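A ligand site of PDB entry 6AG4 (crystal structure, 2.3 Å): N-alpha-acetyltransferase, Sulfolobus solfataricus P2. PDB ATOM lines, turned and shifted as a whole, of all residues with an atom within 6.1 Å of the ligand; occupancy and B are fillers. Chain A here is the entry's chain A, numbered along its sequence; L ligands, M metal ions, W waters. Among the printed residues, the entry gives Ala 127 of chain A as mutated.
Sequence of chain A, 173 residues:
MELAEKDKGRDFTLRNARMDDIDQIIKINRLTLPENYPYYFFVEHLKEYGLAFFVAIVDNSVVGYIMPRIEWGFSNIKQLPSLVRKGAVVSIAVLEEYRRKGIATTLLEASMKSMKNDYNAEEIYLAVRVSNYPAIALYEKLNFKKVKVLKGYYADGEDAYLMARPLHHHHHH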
ATOM      1  N   THR A  32     -17.911 -22.637 -18.081  1.00  0.00           N
ATOM      2  CA  THR A  32     -17.666 -21.924 -16.837  1.00  0.00           C
ATOM      3  C   THR A  32     -17.400 -20.450 -17.057  1.00  0.00           C
ATOM      4  O   THR A  32     -17.501 -19.644 -16.134  1.00  0.00           O
ATOM      5  CB  THR A  32     -16.477 -22.560 -16.095  1.00  0.00           C
ATOM      6  OG1 THR A  32     -15.288 -22.401 -16.888  1.00  0.00           O
ATOM      7  CG2 THR A  32     -16.727 -24.049 -15.864  1.00  0.00           C
ATOM      8  N   LEU A  33     -17.059 -20.088 -18.288  1.00  0.00           N
ATOM      9  CA  LEU A  33     -16.554 -18.742 -18.572  1.00  0.00           C
ATOM     10  C   LEU A  33     -17.179 -18.137 -19.804  1.00  0.00           C
ATOM     11  O   LEU A  33     -17.409 -18.836 -20.798  1.00  0.00           O
ATOM     12  CB  LEU A  33     -15.046 -18.782 -18.757  1.00  0.00           C
ATOM     13  CG  LEU A  33     -14.204 -18.982 -17.498  1.00  0.00           C
ATOM     14  CD1 LEU A  33     -12.736 -19.183 -17.898  1.00  0.00           C
ATOM     15  CD2 LEU A  33     -14.376 -17.798 -16.560  1.00  0.00           C
ATOM     16  N   TYR A  37     -12.053 -18.610 -25.878  1.00  0.00           N
ATOM     17  CA  TYR A  37     -10.992 -18.515 -26.858  1.00  0.00           C
ATOM     18  C   TYR A  37     -11.061 -19.635 -27.894  1.00  0.00           C
ATOM     19  O   TYR A  37     -11.353 -20.779 -27.548  1.00  0.00           O
ATOM     20  CB  TYR A  37      -9.638 -18.531 -26.147  1.00  0.00           C
ATOM     21  CG  TYR A  37      -9.547 -17.585 -24.963  1.00  0.00           C
ATOM     22  CD1 TYR A  37      -9.258 -16.241 -25.155  1.00  0.00           C
ATOM     23  CD2 TYR A  37      -9.718 -18.047 -23.668  1.00  0.00           C
ATOM     24  CE1 TYR A  37      -9.167 -15.369 -24.073  1.00  0.00           C
ATOM     25  CE2 TYR A  37      -9.624 -17.184 -22.576  1.00  0.00           C
ATOM     26  CZ  TYR A  37      -9.353 -15.847 -22.789  1.00  0.00           C
ATOM     27  OH  TYR A  37      -9.272 -14.978 -21.717  1.00  0.00           O
ATOM     28  N   VAL A  89      -1.918 -15.070 -15.749  1.00  0.00           N
ATOM     29  CA  VAL A  89      -2.939 -16.087 -15.768  1.00  0.00           C
ATOM     30  C   VAL A  89      -3.937 -15.678 -16.838  1.00  0.00           C
ATOM     31  O   VAL A  89      -4.747 -14.788 -16.630  1.00  0.00           O
ATOM     32  CB  VAL A  89      -3.630 -16.224 -14.415  1.00  0.00           C
ATOM     33  CG1 VAL A  89      -4.750 -17.285 -14.479  1.00  0.00           C
ATOM     34  CG2 VAL A  89      -2.611 -16.540 -13.343  1.00  0.00           C
ATOM     35  N   VAL A  90      -3.835 -16.302 -18.008  1.00  0.00           N
ATOM     36  CA  VAL A  90      -4.745 -15.989 -19.106  1.00  0.00           C
ATOM     37  C   VAL A  90      -6.156 -16.509 -18.809  1.00  0.00           C
ATOM     38  O   VAL A  90      -7.149 -15.829 -19.043  1.00  0.00           O
ATOM     39  CB  VAL A  90      -4.255 -16.581 -20.431  1.00  0.00           C
ATOM     40  CG1 VAL A  90      -5.128 -16.127 -21.586  1.00  0.00           C
ATOM     41  CG2 VAL A  90      -2.816 -16.178 -20.660  1.00  0.00           C
ATOM     42  N   SER A  91      -6.228 -17.726 -18.306  1.00  0.00           N
ATOM     43  CA  SER A  91      -7.519 -18.320 -17.986  1.00  0.00           C
ATOM     44  C   SER A  91      -7.370 -19.442 -16.982  1.00  0.00           C
ATOM     45  O   SER A  91      -6.391 -20.199 -17.021  1.00  0.00           O
ATOM     46  CB  SER A  91      -8.206 -18.829 -19.253  1.00  0.00           C
ATOM     47  OG  SER A  91      -9.501 -19.319 -18.961  1.00  0.00           O
ATOM     48  N   ILE A  92      -8.336 -19.555 -16.070  1.00  0.00           N
ATOM     49  CA  ILE A  92      -8.373 -20.656 -15.133  1.00  0.00           C
ATOM     50  C   ILE A  92      -9.826 -21.001 -14.794  1.00  0.00           C
ATOM     51  O   ILE A  92     -10.667 -20.111 -14.617  1.00  0.00           O
ATOM     52  CB  ILE A  92      -7.588 -20.336 -13.846  1.00  0.00           C
ATOM     53  CG1 ILE A  92      -7.658 -21.523 -12.892  1.00  0.00           C
ATOM     54  CG2 ILE A  92      -8.131 -19.090 -13.150  1.00  0.00           C
ATOM     55  CD1 ILE A  92      -6.795 -21.355 -11.665  1.00  0.00           C
ATOM     56  N   ALA A  93     -10.127 -22.295 -14.741  1.00  0.00           N
ATOM     57  CA  ALA A  93     -11.470 -22.738 -14.430  1.00  0.00           C
ATOM     58  C   ALA A  93     -11.463 -24.129 -13.847  1.00  0.00           C
ATOM     59  O   ALA A  93     -10.646 -24.983 -14.225  1.00  0.00           O
ATOM     60  CB  ALA A  93     -12.355 -22.691 -15.663  1.00  0.00           C
ATOM     61  N   VAL A  94     -12.371 -24.349 -12.905  1.00  0.00           N
ATOM     62  CA  VAL A  94     -12.611 -25.668 -12.350  1.00  0.00           C
ATOM     63  C   VAL A  94     -14.098 -25.978 -12.492  1.00  0.00           C
ATOM     64  O   VAL A  94     -14.934 -25.119 -12.176  1.00  0.00           O
ATOM     65  CB  VAL A  94     -12.177 -25.759 -10.885  1.00  0.00           C
ATOM     66  CG1 VAL A  94     -12.528 -27.127 -10.305  1.00  0.00           C
ATOM     67  CG2 VAL A  94     -10.674 -25.495 -10.753  1.00  0.00           C
ATOM     68  N   LEU A  95     -14.420 -27.170 -12.999  1.00  0.00           N
ATOM     69  CA  LEU A  95     -15.811 -27.574 -13.129  1.00  0.00           C
ATOM     70  C   LEU A  95     -16.505 -27.520 -11.783  1.00  0.00           C
ATOM     71  O   LEU A  95     -15.932 -27.919 -10.768  1.00  0.00           O
ATOM     72  CB  LEU A  95     -15.926 -28.978 -13.732  1.00  0.00           C
ATOM     73  CG  LEU A  95     -15.741 -29.071 -15.239  1.00  0.00           C
ATOM     74  CD1 LEU A  95     -15.740 -30.531 -15.659  1.00  0.00           C
ATOM     75  CD2 LEU A  95     -16.847 -28.310 -15.965  1.00  0.00           C
ATOM     76  N   TYR A  98     -16.399 -30.027  -8.877  1.00  0.00           N
ATOM     77  CA  TYR A  98     -15.186 -30.284  -8.106  1.00  0.00           C
ATOM     78  C   TYR A  98     -14.618 -29.029  -7.439  1.00  0.00           C
ATOM     79  O   TYR A  98     -13.432 -28.974  -7.113  1.00  0.00           O
ATOM     80  CB  TYR A  98     -14.133 -30.935  -8.991  1.00  0.00           C
ATOM     81  CG  TYR A  98     -14.620 -32.216  -9.606  1.00  0.00           C
ATOM     82  CD1 TYR A  98     -14.499 -33.429  -8.935  1.00  0.00           C
ATOM     83  CD2 TYR A  98     -15.222 -32.217 -10.859  1.00  0.00           C
ATOM     84  CE1 TYR A  98     -14.967 -34.618  -9.507  1.00  0.00           C
ATOM     85  CE2 TYR A  98     -15.684 -33.394 -11.431  1.00  0.00           C
ATOM     86  CZ  TYR A  98     -15.551 -34.582 -10.749  1.00  0.00           C
ATOM     87  OH  TYR A  98     -16.014 -35.758 -11.321  1.00  0.00           O
ATOM     88  N   ARG A  99     -15.466 -28.035  -7.210  1.00  0.00           N
ATOM     89  CA  ARG A  99     -14.983 -26.798  -6.626  1.00  0.00           C
ATOM     90  C   ARG A  99     -14.851 -26.912  -5.102  1.00  0.00           C
ATOM     91  O   ARG A  99     -15.365 -27.850  -4.490  1.00  0.00           O
ATOM     92  CB  ARG A  99     -15.905 -25.636  -7.008  1.00  0.00           C
ATOM     93  CG  ARG A  99     -15.705 -25.206  -8.463  1.00  0.00           C
ATOM     94  CD  ARG A  99     -16.635 -24.078  -8.885  1.00  0.00           C
ATOM     95  NE  ARG A  99     -16.534 -23.851 -10.328  1.00  0.00           N
ATOM     96  CZ  ARG A  99     -17.422 -23.194 -11.068  1.00  0.00           C
ATOM     97  NH1 ARG A  99     -18.512 -22.670 -10.508  1.00  0.00           N
ATOM     98  NH2 ARG A  99     -17.217 -23.070 -12.369  1.00  0.00           N
ATOM     99  N   ARG A 100     -14.114 -25.978  -4.505  1.00  0.00           N
ATOM    100  CA  ARG A 100     -13.894 -25.942  -3.055  1.00  0.00           C
ATOM    101  C   ARG A 100     -13.156 -27.170  -2.532  1.00  0.00           C
ATOM    102  O   ARG A 100     -13.375 -27.595  -1.398  1.00  0.00           O
ATOM    103  CB  ARG A 100     -15.222 -25.790  -2.301  1.00  0.00           C
ATOM    104  CG  ARG A 100     -16.019 -24.562  -2.696  1.00  0.00           C
ATOM    105  CD  ARG A 100     -15.185 -23.282  -2.709  1.00  0.00           C
ATOM    106  NE  ARG A 100     -14.806 -22.809  -1.374  1.00  0.00           N
ATOM    107  CZ  ARG A 100     -15.604 -22.088  -0.578  1.00  0.00           C
ATOM    108  NH1 ARG A 100     -16.838 -21.789  -0.969  1.00  0.00           N
ATOM    109  NH2 ARG A 100     -15.171 -21.690   0.607  1.00  0.00           N
ATOM    110  N   LYS A 101     -12.249 -27.715  -3.350  1.00  0.00           N
ATOM    111  CA  LYS A 101     -11.451 -28.857  -2.943  1.00  0.00           C
ATOM    112  C   LYS A 101      -9.978 -28.518  -2.961  1.00  0.00           C
ATOM    113  O   LYS A 101      -9.142 -29.340  -2.607  1.00  0.00           O
ATOM    114  CB  LYS A 101     -11.711 -30.055  -3.848  1.00  0.00           C
ATOM    115  CG  LYS A 101     -13.115 -30.636  -3.692  1.00  0.00           C
ATOM    116  CD  LYS A 101     -13.598 -31.242  -4.984  1.00  0.00           C
ATOM    117  CE  LYS A 101     -13.495 -32.743  -4.960  1.00  0.00           C
ATOM    118  NZ  LYS A 101     -14.855 -33.350  -4.883  1.00  0.00           N
ATOM    119  N   GLY A 102      -9.669 -27.293  -3.385  1.00  0.00           N
ATOM    120  CA  GLY A 102      -8.316 -26.796  -3.385  1.00  0.00           C
ATOM    121  C   GLY A 102      -7.684 -26.881  -4.754  1.00  0.00           C
ATOM    122  O   GLY A 102      -6.489 -26.639  -4.905  1.00  0.00           O
ATOM    123  N   ILE A 103      -8.495 -27.223  -5.762  1.00  0.00           N
ATOM    124  CA  ILE A 103      -7.944 -27.444  -7.107  1.00  0.00           C
ATOM    125  C   ILE A 103      -7.439 -26.169  -7.773  1.00  0.00           C
ATOM    126  O   ILE A 103      -6.336 -26.158  -8.332  1.00  0.00           O
ATOM    127  CB  ILE A 103      -8.951 -28.110  -8.039  1.00  0.00           C
ATOM    128  CG1 ILE A 103      -9.283 -29.524  -7.530  1.00  0.00           C
ATOM    129  CG2 ILE A 103      -8.403 -28.193  -9.452  1.00  0.00           C
ATOM    130  CD1 ILE A 103     -10.104 -30.325  -8.498  1.00  0.00           C
ATOM    131  N   ALA A 104      -8.225 -25.089  -7.721  1.00  0.00           N
ATOM    132  CA  ALA A 104      -7.763 -23.851  -8.339  1.00  0.00           C
ATOM    133  C   ALA A 104      -6.467 -23.368  -7.660  1.00  0.00           C
ATOM    134  O   ALA A 104      -5.554 -22.925  -8.328  1.00  0.00           O
ATOM    135  CB  ALA A 104      -8.840 -22.789  -8.277  1.00  0.00           C
ATOM    136  N   THR A 105      -6.411 -23.485  -6.339  1.00  0.00           N
ATOM    137  CA  THR A 105      -5.234 -23.129  -5.557  1.00  0.00           C
ATOM    138  C   THR A 105      -4.017 -23.938  -5.989  1.00  0.00           C
ATOM    139  O   THR A 105      -2.961 -23.384  -6.208  1.00  0.00           O
ATOM    140  CB  THR A 105      -5.498 -23.349  -4.060  1.00  0.00           C
ATOM    141  OG1 THR A 105      -6.523 -22.452  -3.630  1.00  0.00           O
ATOM    142  CG2 THR A 105      -4.230 -23.110  -3.217  1.00  0.00           C
ATOM    143  N   THR A 106      -4.196 -25.251  -6.122  1.00  0.00           N
ATOM    144  CA  THR A 106      -3.104 -26.135  -6.520  1.00  0.00           C
ATOM    145  C   THR A 106      -2.619 -25.827  -7.927  1.00  0.00           C
ATOM    146  O   THR A 106      -1.416 -25.805  -8.192  1.00  0.00           O
ATOM    147  CB  THR A 106      -3.523 -27.609  -6.435  1.00  0.00           C
ATOM    148  OG1 THR A 106      -4.242 -27.829  -5.215  1.00  0.00           O
ATOM    149  CG2 THR A 106      -2.323 -28.512  -6.459  1.00  0.00           C
ATOM    150  N   LEU A 126      -3.088 -10.866 -13.405  1.00  0.00           N
ATOM    151  CA  LEU A 126      -4.273 -11.299 -14.119  1.00  0.00           C
ATOM    152  C   LEU A 126      -5.314 -10.182 -14.085  1.00  0.00           C
ATOM    153  O   LEU A 126      -5.132  -9.158 -13.407  1.00  0.00           O
ATOM    154  CB  LEU A 126      -4.845 -12.587 -13.496  1.00  0.00           C
ATOM    155  CG  LEU A 126      -5.143 -12.533 -11.995  1.00  0.00           C
ATOM    156  CD1 LEU A 126      -6.526 -11.931 -11.654  1.00  0.00           C
ATOM    157  CD2 LEU A 126      -4.982 -13.912 -11.366  1.00  0.00           C
ATOM    158  N   ALA A 127      -6.384 -10.394 -14.850  1.00  0.00           N
ATOM    159  CA  ALA A 127      -7.570  -9.561 -14.807  1.00  0.00           C
ATOM    160  C   ALA A 127      -8.747 -10.403 -14.358  1.00  0.00           C
ATOM    161  O   ALA A 127      -8.869 -11.578 -14.737  1.00  0.00           O
ATOM    162  CB  ALA A 127      -7.851  -8.951 -16.167  1.00  0.00           C
ATOM    163  N   VAL A 128      -9.598  -9.840 -13.517  1.00  0.00           N
ATOM    164  CA  VAL A 128     -10.778 -10.555 -13.065  1.00  0.00           C
ATOM    165  C   VAL A 128     -11.978  -9.600 -12.961  1.00  0.00           C
ATOM    166  O   VAL A 128     -11.816  -8.411 -12.640  1.00  0.00           O
ATOM    167  CB  VAL A 128     -10.488 -11.247 -11.718  1.00  0.00           C
ATOM    168  CG1 VAL A 128     -10.067 -10.227 -10.660  1.00  0.00           C
ATOM    169  CG2 VAL A 128     -11.704 -12.040 -11.259  1.00  0.00           C
ATOM    170  N   ARG A 129     -13.167 -10.102 -13.276  1.00  0.00           N
ATOM    171  CA  ARG A 129     -14.383  -9.280 -13.184  1.00  0.00           C
ATOM    172  C   ARG A 129     -14.597  -8.761 -11.770  1.00  0.00           C
ATOM    173  O   ARG A 129     -14.403  -9.494 -10.807  1.00  0.00           O
ATOM    174  CB  ARG A 129     -15.606 -10.089 -13.637  1.00  0.00           C
ATOM    175  CG  ARG A 129     -15.579 -10.493 -15.095  1.00  0.00           C
ATOM    176  CD  ARG A 129     -16.853 -11.193 -15.527  1.00  0.00           C
ATOM    177  NE  ARG A 129     -16.800 -11.525 -16.943  1.00  0.00           N
ATOM    178  CZ  ARG A 129     -17.471 -10.885 -17.896  1.00  0.00           C
ATOM    179  NH1 ARG A 129     -18.284  -9.880 -17.586  1.00  0.00           N
ATOM    180  NH2 ARG A 129     -17.344 -11.266 -19.160  1.00  0.00           N
ATOM    181  N   ASN A 132     -16.797 -10.992  -9.776  1.00  0.00           N
ATOM    182  CA  ASN A 132     -16.407 -12.393  -9.610  1.00  0.00           C
ATOM    183  C   ASN A 132     -15.756 -12.576  -8.248  1.00  0.00           C
ATOM    184  O   ASN A 132     -14.532 -12.782  -8.126  1.00  0.00           O
ATOM    185  CB  ASN A 132     -15.449 -12.832 -10.724  1.00  0.00           C
ATOM    186  CG  ASN A 132     -15.267 -14.337 -10.798  1.00  0.00           C
ATOM    187  OD1 ASN A 132     -15.663 -15.076  -9.887  1.00  0.00           O
ATOM    188  ND2 ASN A 132     -14.652 -14.802 -11.875  1.00  0.00           N
ATOM    189  N   TYR A 133     -16.584 -12.494  -7.206  1.00  0.00           N
ATOM    190  CA  TYR A 133     -16.123 -12.532  -5.828  1.00  0.00           C
ATOM    191  C   TYR A 133     -15.448 -13.846  -5.370  1.00  0.00           C
ATOM    192  O   TYR A 133     -14.504 -13.795  -4.573  1.00  0.00           O
ATOM    193  CB  TYR A 133     -17.308 -12.204  -4.915  1.00  0.00           C
ATOM    194  CG  TYR A 133     -17.808 -10.788  -5.115  1.00  0.00           C
ATOM    195  CD1 TYR A 133     -17.016  -9.706  -4.763  1.00  0.00           C
ATOM    196  CD2 TYR A 133     -19.051 -10.532  -5.687  1.00  0.00           C
ATOM    197  CE1 TYR A 133     -17.458  -8.397  -4.944  1.00  0.00           C
ATOM    198  CE2 TYR A 133     -19.502  -9.227  -5.867  1.00  0.00           C
ATOM    199  CZ  TYR A 133     -18.691  -8.170  -5.505  1.00  0.00           C
ATOM    200  OH  TYR A 133     -19.136  -6.883  -5.686  1.00  0.00           O
ATOM    201  N   PRO A 134     -15.910 -15.002  -5.861  1.00  0.00           N
ATOM    202  CA  PRO A 134     -15.142 -16.228  -5.567  1.00  0.00           C
ATOM    203  C   PRO A 134     -13.696 -16.203  -6.063  1.00  0.00           C
ATOM    204  O   PRO A 134     -12.811 -16.522  -5.296  1.00  0.00           O
ATOM    205  CB  PRO A 134     -15.935 -17.319  -6.289  1.00  0.00           C
ATOM    206  CG  PRO A 134     -17.364 -16.826  -6.212  1.00  0.00           C
ATOM    207  CD  PRO A 134     -17.239 -15.317  -6.427  1.00  0.00           C
ATOM    208  N   ALA A 135     -13.459 -15.814  -7.317  1.00  0.00           N
ATOM    209  CA  ALA A 135     -12.098 -15.723  -7.855  1.00  0.00           C
ATOM    210  C   ALA A 135     -11.270 -14.673  -7.122  1.00  0.00           C
ATOM    211  O   ALA A 135     -10.104 -14.922  -6.783  1.00  0.00           O
ATOM    212  CB  ALA A 135     -12.127 -15.425  -9.331  1.00  0.00           C
ATOM    213  N   ALA A 137     -11.588 -13.640  -4.080  1.00  0.00           N
ATOM    214  CA  ALA A 137     -11.236 -14.257  -2.809  1.00  0.00           C
ATOM    215  C   ALA A 137     -10.075 -15.247  -2.955  1.00  0.00           C
ATOM    216  O   ALA A 137      -9.153 -15.256  -2.151  1.00  0.00           O
ATOM    217  CB  ALA A 137     -12.458 -14.936  -2.187  1.00  0.00           C
ATOM    218  N   LEU A 138     -10.133 -16.097  -3.986  1.00  0.00           N
ATOM    219  CA  LEU A 138      -9.050 -17.029  -4.275  1.00  0.00           C
ATOM    220  C   LEU A 138      -7.716 -16.303  -4.460  1.00  0.00           C
ATOM    221  O   LEU A 138      -6.716 -16.634  -3.819  1.00  0.00           O
ATOM    222  CB  LEU A 138      -9.366 -17.841  -5.524  1.00  0.00           C
ATOM    223  CG  LEU A 138      -8.240 -18.670  -6.149  1.00  0.00           C
ATOM    224  CD1 LEU A 138      -7.932 -19.893  -5.312  1.00  0.00           C
ATOM    225  CD2 LEU A 138      -8.607 -19.075  -7.583  1.00  0.00           C
ATOM    226  N   TYR A 139      -7.722 -15.302  -5.331  1.00  0.00           N
ATOM    227  CA  TYR A 139      -6.514 -14.588  -5.692  1.00  0.00           C
ATOM    228  C   TYR A 139      -5.955 -13.891  -4.466  1.00  0.00           C
ATOM    229  O   TYR A 139      -4.764 -13.993  -4.193  1.00  0.00           O
ATOM    230  CB  TYR A 139      -6.804 -13.590  -6.823  1.00  0.00           C
ATOM    231  CG  TYR A 139      -7.258 -14.281  -8.085  1.00  0.00           C
ATOM    232  CD1 TYR A 139      -6.717 -15.498  -8.470  1.00  0.00           C
ATOM    233  CD2 TYR A 139      -8.266 -13.730  -8.873  1.00  0.00           C
ATOM    234  CE1 TYR A 139      -7.129 -16.144  -9.620  1.00  0.00           C
ATOM    235  CE2 TYR A 139      -8.703 -14.363 -10.023  1.00  0.00           C
ATOM    236  CZ  TYR A 139      -8.135 -15.570 -10.386  1.00  0.00           C
ATOM    237  OH  TYR A 139      -8.559 -16.210 -11.536  1.00  0.00           O
ATOM    238  N   LYS A 141      -6.262 -14.679  -1.350  1.00  0.00           N
ATOM    239  CA  LYS A 141      -5.656 -15.670  -0.457  1.00  0.00           C
ATOM    240  C   LYS A 141      -4.275 -16.123  -0.945  1.00  0.00           C
ATOM    241  O   LYS A 141      -3.497 -16.682  -0.187  1.00  0.00           O
ATOM    242  CB  LYS A 141      -6.569 -16.893  -0.306  1.00  0.00           C
ATOM    243  CG  LYS A 141      -7.677 -16.708   0.718  1.00  0.00           C
ATOM    244  CD  LYS A 141      -8.218 -18.037   1.211  1.00  0.00           C
ATOM    245  CE  LYS A 141      -9.085 -17.874   2.473  1.00  0.00           C
ATOM    246  NZ  LYS A 141      -9.784 -16.562   2.574  1.00  0.00           N
ATOM    247  N   TYR A 154     -14.288  -5.983 -20.170  1.00  0.00           N
ATOM    248  CA  TYR A 154     -14.938  -7.173 -20.719  1.00  0.00           C
ATOM    249  C   TYR A 154     -15.943  -6.862 -21.811  1.00  0.00           C
ATOM    250  O   TYR A 154     -16.449  -5.746 -21.897  1.00  0.00           O
ATOM    251  CB  TYR A 154     -15.613  -7.960 -19.599  1.00  0.00           C
ATOM    252  CG  TYR A 154     -14.608  -8.609 -18.684  1.00  0.00           C
ATOM    253  CD1 TYR A 154     -14.044  -9.839 -18.998  1.00  0.00           C
ATOM    254  CD2 TYR A 154     -14.188  -7.960 -17.524  1.00  0.00           C
ATOM    255  CE1 TYR A 154     -13.120 -10.432 -18.165  1.00  0.00           C
ATOM    256  CE2 TYR A 154     -13.253  -8.549 -16.690  1.00  0.00           C
ATOM    257  CZ  TYR A 154     -12.721  -9.780 -17.006  1.00  0.00           C
ATOM    258  OH  TYR A 154     -11.787 -10.369 -16.182  1.00  0.00           O
HETATM  259  N1  LIG L   1     -16.925 -18.585  -2.418  1.00  0.00           N
HETATM  260  C1  LIG L   1     -16.125 -17.993  -1.466  1.00  0.00           C
HETATM  261  N2  LIG L   1     -14.773 -18.184  -1.479  1.00  0.00           N
HETATM  262  C2  LIG L   1     -14.214 -18.988  -2.455  1.00  0.00           C
HETATM  263  C3  LIG L   1     -15.005 -19.578  -3.378  1.00  0.00           C
HETATM  264  C4  LIG L   1     -16.382 -19.374  -3.365  1.00  0.00           C
HETATM  265  N3  LIG L   1     -17.425 -19.810  -4.143  1.00  0.00           N
HETATM  266  N4  LIG L   1     -14.206 -20.297  -4.203  1.00  0.00           N
HETATM  267  C5  LIG L   1     -12.935 -20.160  -3.793  1.00  0.00           C
HETATM  268  N5  LIG L   1     -12.933 -19.340  -2.705  1.00  0.00           N
HETATM  269  C6  LIG L   1     -11.763 -18.986  -1.983  1.00  0.00           C
HETATM  270  C7  LIG L   1     -11.867 -19.509  -0.747  1.00  0.00           C
HETATM  271  O1  LIG L   1     -11.248 -18.652   0.255  1.00  0.00           O
HETATM  272  C8  LIG L   1     -11.114 -20.855  -0.826  1.00  0.00           C
HETATM  273  O2  LIG L   1     -10.638 -21.216   0.385  1.00  0.00           O
HETATM  274  P1  LIG L   1     -11.432 -22.349   1.203  1.00  0.00           P
HETATM  275  O3  LIG L   1     -10.472 -23.256   1.821  1.00  0.00           O
HETATM  276  O4  LIG L   1     -12.297 -21.686   2.276  1.00  0.00           O
HETATM  277  O5  LIG L   1     -12.352 -23.143   0.252  1.00  0.00           O
HETATM  278  C9  LIG L   1      -9.952 -20.534  -1.827  1.00  0.00           C
HETATM  279  O6  LIG L   1     -10.490 -19.710  -2.691  1.00  0.00           O
HETATM  280  C10 LIG L   1      -9.450 -21.784  -2.505  1.00  0.00           C
HETATM  281  O7  LIG L   1     -10.510 -22.428  -3.168  1.00  0.00           O
HETATM  282  P2  LIG L   1     -10.266 -23.457  -4.331  1.00  0.00           P
HETATM  283  O8  LIG L   1     -10.877 -24.789  -3.910  1.00  0.00           O
HETATM  284  O9  LIG L   1      -8.770 -23.628  -4.639  1.00  0.00           O
HETATM  285  O10 LIG L   1     -10.986 -22.875  -5.617  1.00  0.00           O
HETATM  286  P3  LIG L   1     -11.834 -23.770  -6.668  1.00  0.00           P
HETATM  287  O11 LIG L   1     -11.087 -25.042  -6.956  1.00  0.00           O
HETATM  288  O12 LIG L   1     -13.186 -24.039  -6.103  1.00  0.00           O
HETATM  289  O13 LIG L   1     -11.998 -22.864  -8.006  1.00  0.00           O
HETATM  290  C11 LIG L   1     -12.576 -20.854  -9.238  1.00  0.00           C
HETATM  291  C12 LIG L   1     -12.042 -21.460  -7.859  1.00  0.00           C
HETATM  292  C13 LIG L   1     -11.461 -21.047 -10.362  1.00  0.00           C
HETATM  293  C14 LIG L   1     -12.815 -19.360  -9.007  1.00  0.00           C
HETATM  294  C15 LIG L   1     -13.853 -21.587  -9.561  1.00  0.00           C
HETATM  295  O14 LIG L   1     -14.905 -21.116  -8.710  1.00  0.00           O
HETATM  296  C16 LIG L   1     -14.329 -21.437 -11.007  1.00  0.00           C
HETATM  297  O15 LIG L   1     -13.930 -22.191 -11.878  1.00  0.00           O
HETATM  298  N6  LIG L   1     -15.269 -20.451 -11.282  1.00  0.00           N
HETATM  299  C17 LIG L   1     -15.802 -20.216 -12.609  1.00  0.00           C
HETATM  300  C18 LIG L   1     -14.645 -19.907 -13.630  1.00  0.00           C
HETATM  301  C19 LIG L   1     -13.917 -18.657 -13.177  1.00  0.00           C
HETATM  302  O16 LIG L   1     -14.582 -17.654 -12.831  1.00  0.00           O
HETATM  303  N7  LIG L   1     -12.449 -18.607 -13.161  1.00  0.00           N
HETATM  304  C20 LIG L   1     -11.732 -17.414 -12.740  1.00  0.00           C
HETATM  305  C21 LIG L   1     -11.840 -16.331 -13.853  1.00  0.00           C
HETATM  306  S1  LIG L   1     -10.590 -15.086 -13.651  1.00  0.00           S
HETATM  307  C22 LIG L   1      -9.389 -15.322 -14.932  1.00  0.00           C
HETATM  308  O17 LIG L   1      -8.217 -15.155 -14.695  1.00  0.00           O
HETATM  309  C23 LIG L   1      -9.791 -16.006 -16.222  1.00  0.00           C
HETATM  310 CA    CA M   1     -13.809 -13.215 -14.274  1.00  0.00          CA
HETATM  311  O   HOH W   1     -16.204 -18.023  -9.947  1.00  0.00           O
HETATM  312  O   HOH W   2     -10.797 -24.962  -0.988  1.00  0.00           O
HETATM  313  O   HOH W   3     -15.041 -22.115  -6.113  1.00  0.00           O
HETATM  314  O   HOH W   4     -11.405 -27.303  -6.013  1.00  0.00           O
HETATM  315  O   HOH W   5     -17.629 -22.466  -5.987  1.00  0.00           O
HETATM  316  O   HOH W   6     -13.732 -17.039   0.885  1.00  0.00           O
HETATM  317  O   HOH W   7     -18.662 -22.693  -2.897  1.00  0.00           O
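N of Gly 102 lies within hydrogen-bond range of O8 of the ligand (2.8 Å).
The side-chain amino group (NZ) of Lys 141 lies close to an oxygen (O1) of the ligand, at 3.4 Å.
The side-chain hydroxyl (OH) of Tyr 139 lies close to a sulfur (S1) of the ligand (3.1 Å).
An oxygen (O5) of the ligand lies within salt-bridge range of the guanidinium group (NE) of Arg 100 (3.0 Å).
An oxygen (O16) of the ligand is in hydrogen-bond range of the side-chain amide nitrogen (ND2) of Asn 132 (3.0 Å).
The backbone NH (N) of Arg 100 sits at hydrogen-bond distance from an oxygen (O12) of the ligand (2.7 Å).
The backbone NH (N) of Ala 104 lies within hydrogen-bond range of an oxygen (O11) of the ligand, 3.0 Å away.
The side-chain hydroxyl (OG1) of Thr 105 sits at hydrogen-bond distance from an oxygen (O9) of the ligand (2.7 Å).
N of Lys 101 is in hydrogen-bond range of O8 of the ligand, 3.3 Å away.
O15 of the ligand lies close to NH2 of Arg 99, 3.4 Å away.
An oxygen (O15) of the ligand lies within hydrogen-bond range of the backbone NH (N) of Val 94, 2.9 Å away.
The backbone NH of Thr 105 sits at hydrogen-bond distance from an oxygen (O9) of the ligand, at 2.9 Å.
A nitrogen (N7) of the ligand sits at hydrogen-bond distance from the backbone carbonyl oxygen of Ile 92, 2.7 Å away.
The side-chain amide oxygen of Asn 132 is in hydrogen-bond range of the backbone NH of Ala 135.
O of Ala 127 sits at hydrogen-bond distance from OH of Tyr 154 (3.5 Å).
O of Gly 102 is in hydrogen-bond range of OG1 of Thr 106 (2.6 Å).
O of Val 94 lies within hydrogen-bond range of NE of Arg 99 (2.8 Å).
Thr 32 touches the ligand (O to C18, 3.8 Å).
Leu 33 touches the ligand (CD2 to C19, 3.5 Å).
O of Val 89 touches O17 of the ligand (3.99 Å).
Val 90 touches the ligand.
Ser 91 touches the ligand.
CA of Ala 93 touches O15 of the ligand, at 3.6 Å.
Ile 103 touches the ligand.
Ala 127 touches the ligand (O to O17, 3.6 Å).
Pro 134 touches the ligand (CB to C4, 3.6 Å).
CA of Ala 135 touches C14 of the ligand (3.9 Å).
CA of Leu 138 touches O6 of the ligand (3.4 Å).
Hydrophobic or aromatic side chains that line the ligand: Leu 33, Ile 92, Val 94, Ile 103, Ala 104, Pro 134, Ala 135 and Leu 138.
22 residues have an atom within 4 Å of the ligand: Thr 32, Leu 33, Val 89, Val 90, Ser 91, Ile 92, Ala 93, Val 94, Arg 99, Arg 100, Lys 101, Gly 102, Ile 103, Ala 104, Thr 105, Ala 127, Asn 132, Pro 134, Ala 135, Leu 138, Tyr 139 and Lys 141.
Along chain A the residues within 4 Å of the ligand span positions 32 to 141.
The nearest printed residue that does not touch the ligand is Val 128 (4.03 Å).
Water W1 lies within hydrogen-bond range of N6 of the ligand (2.9 Å) and OD1 of Asn 132 (3.0 Å).
Water W7 lies within hydrogen-bond range of the guanidinium group of Arg 100 (2.8 Å) and a nitrogen (N3) of the ligand (3.4 Å).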
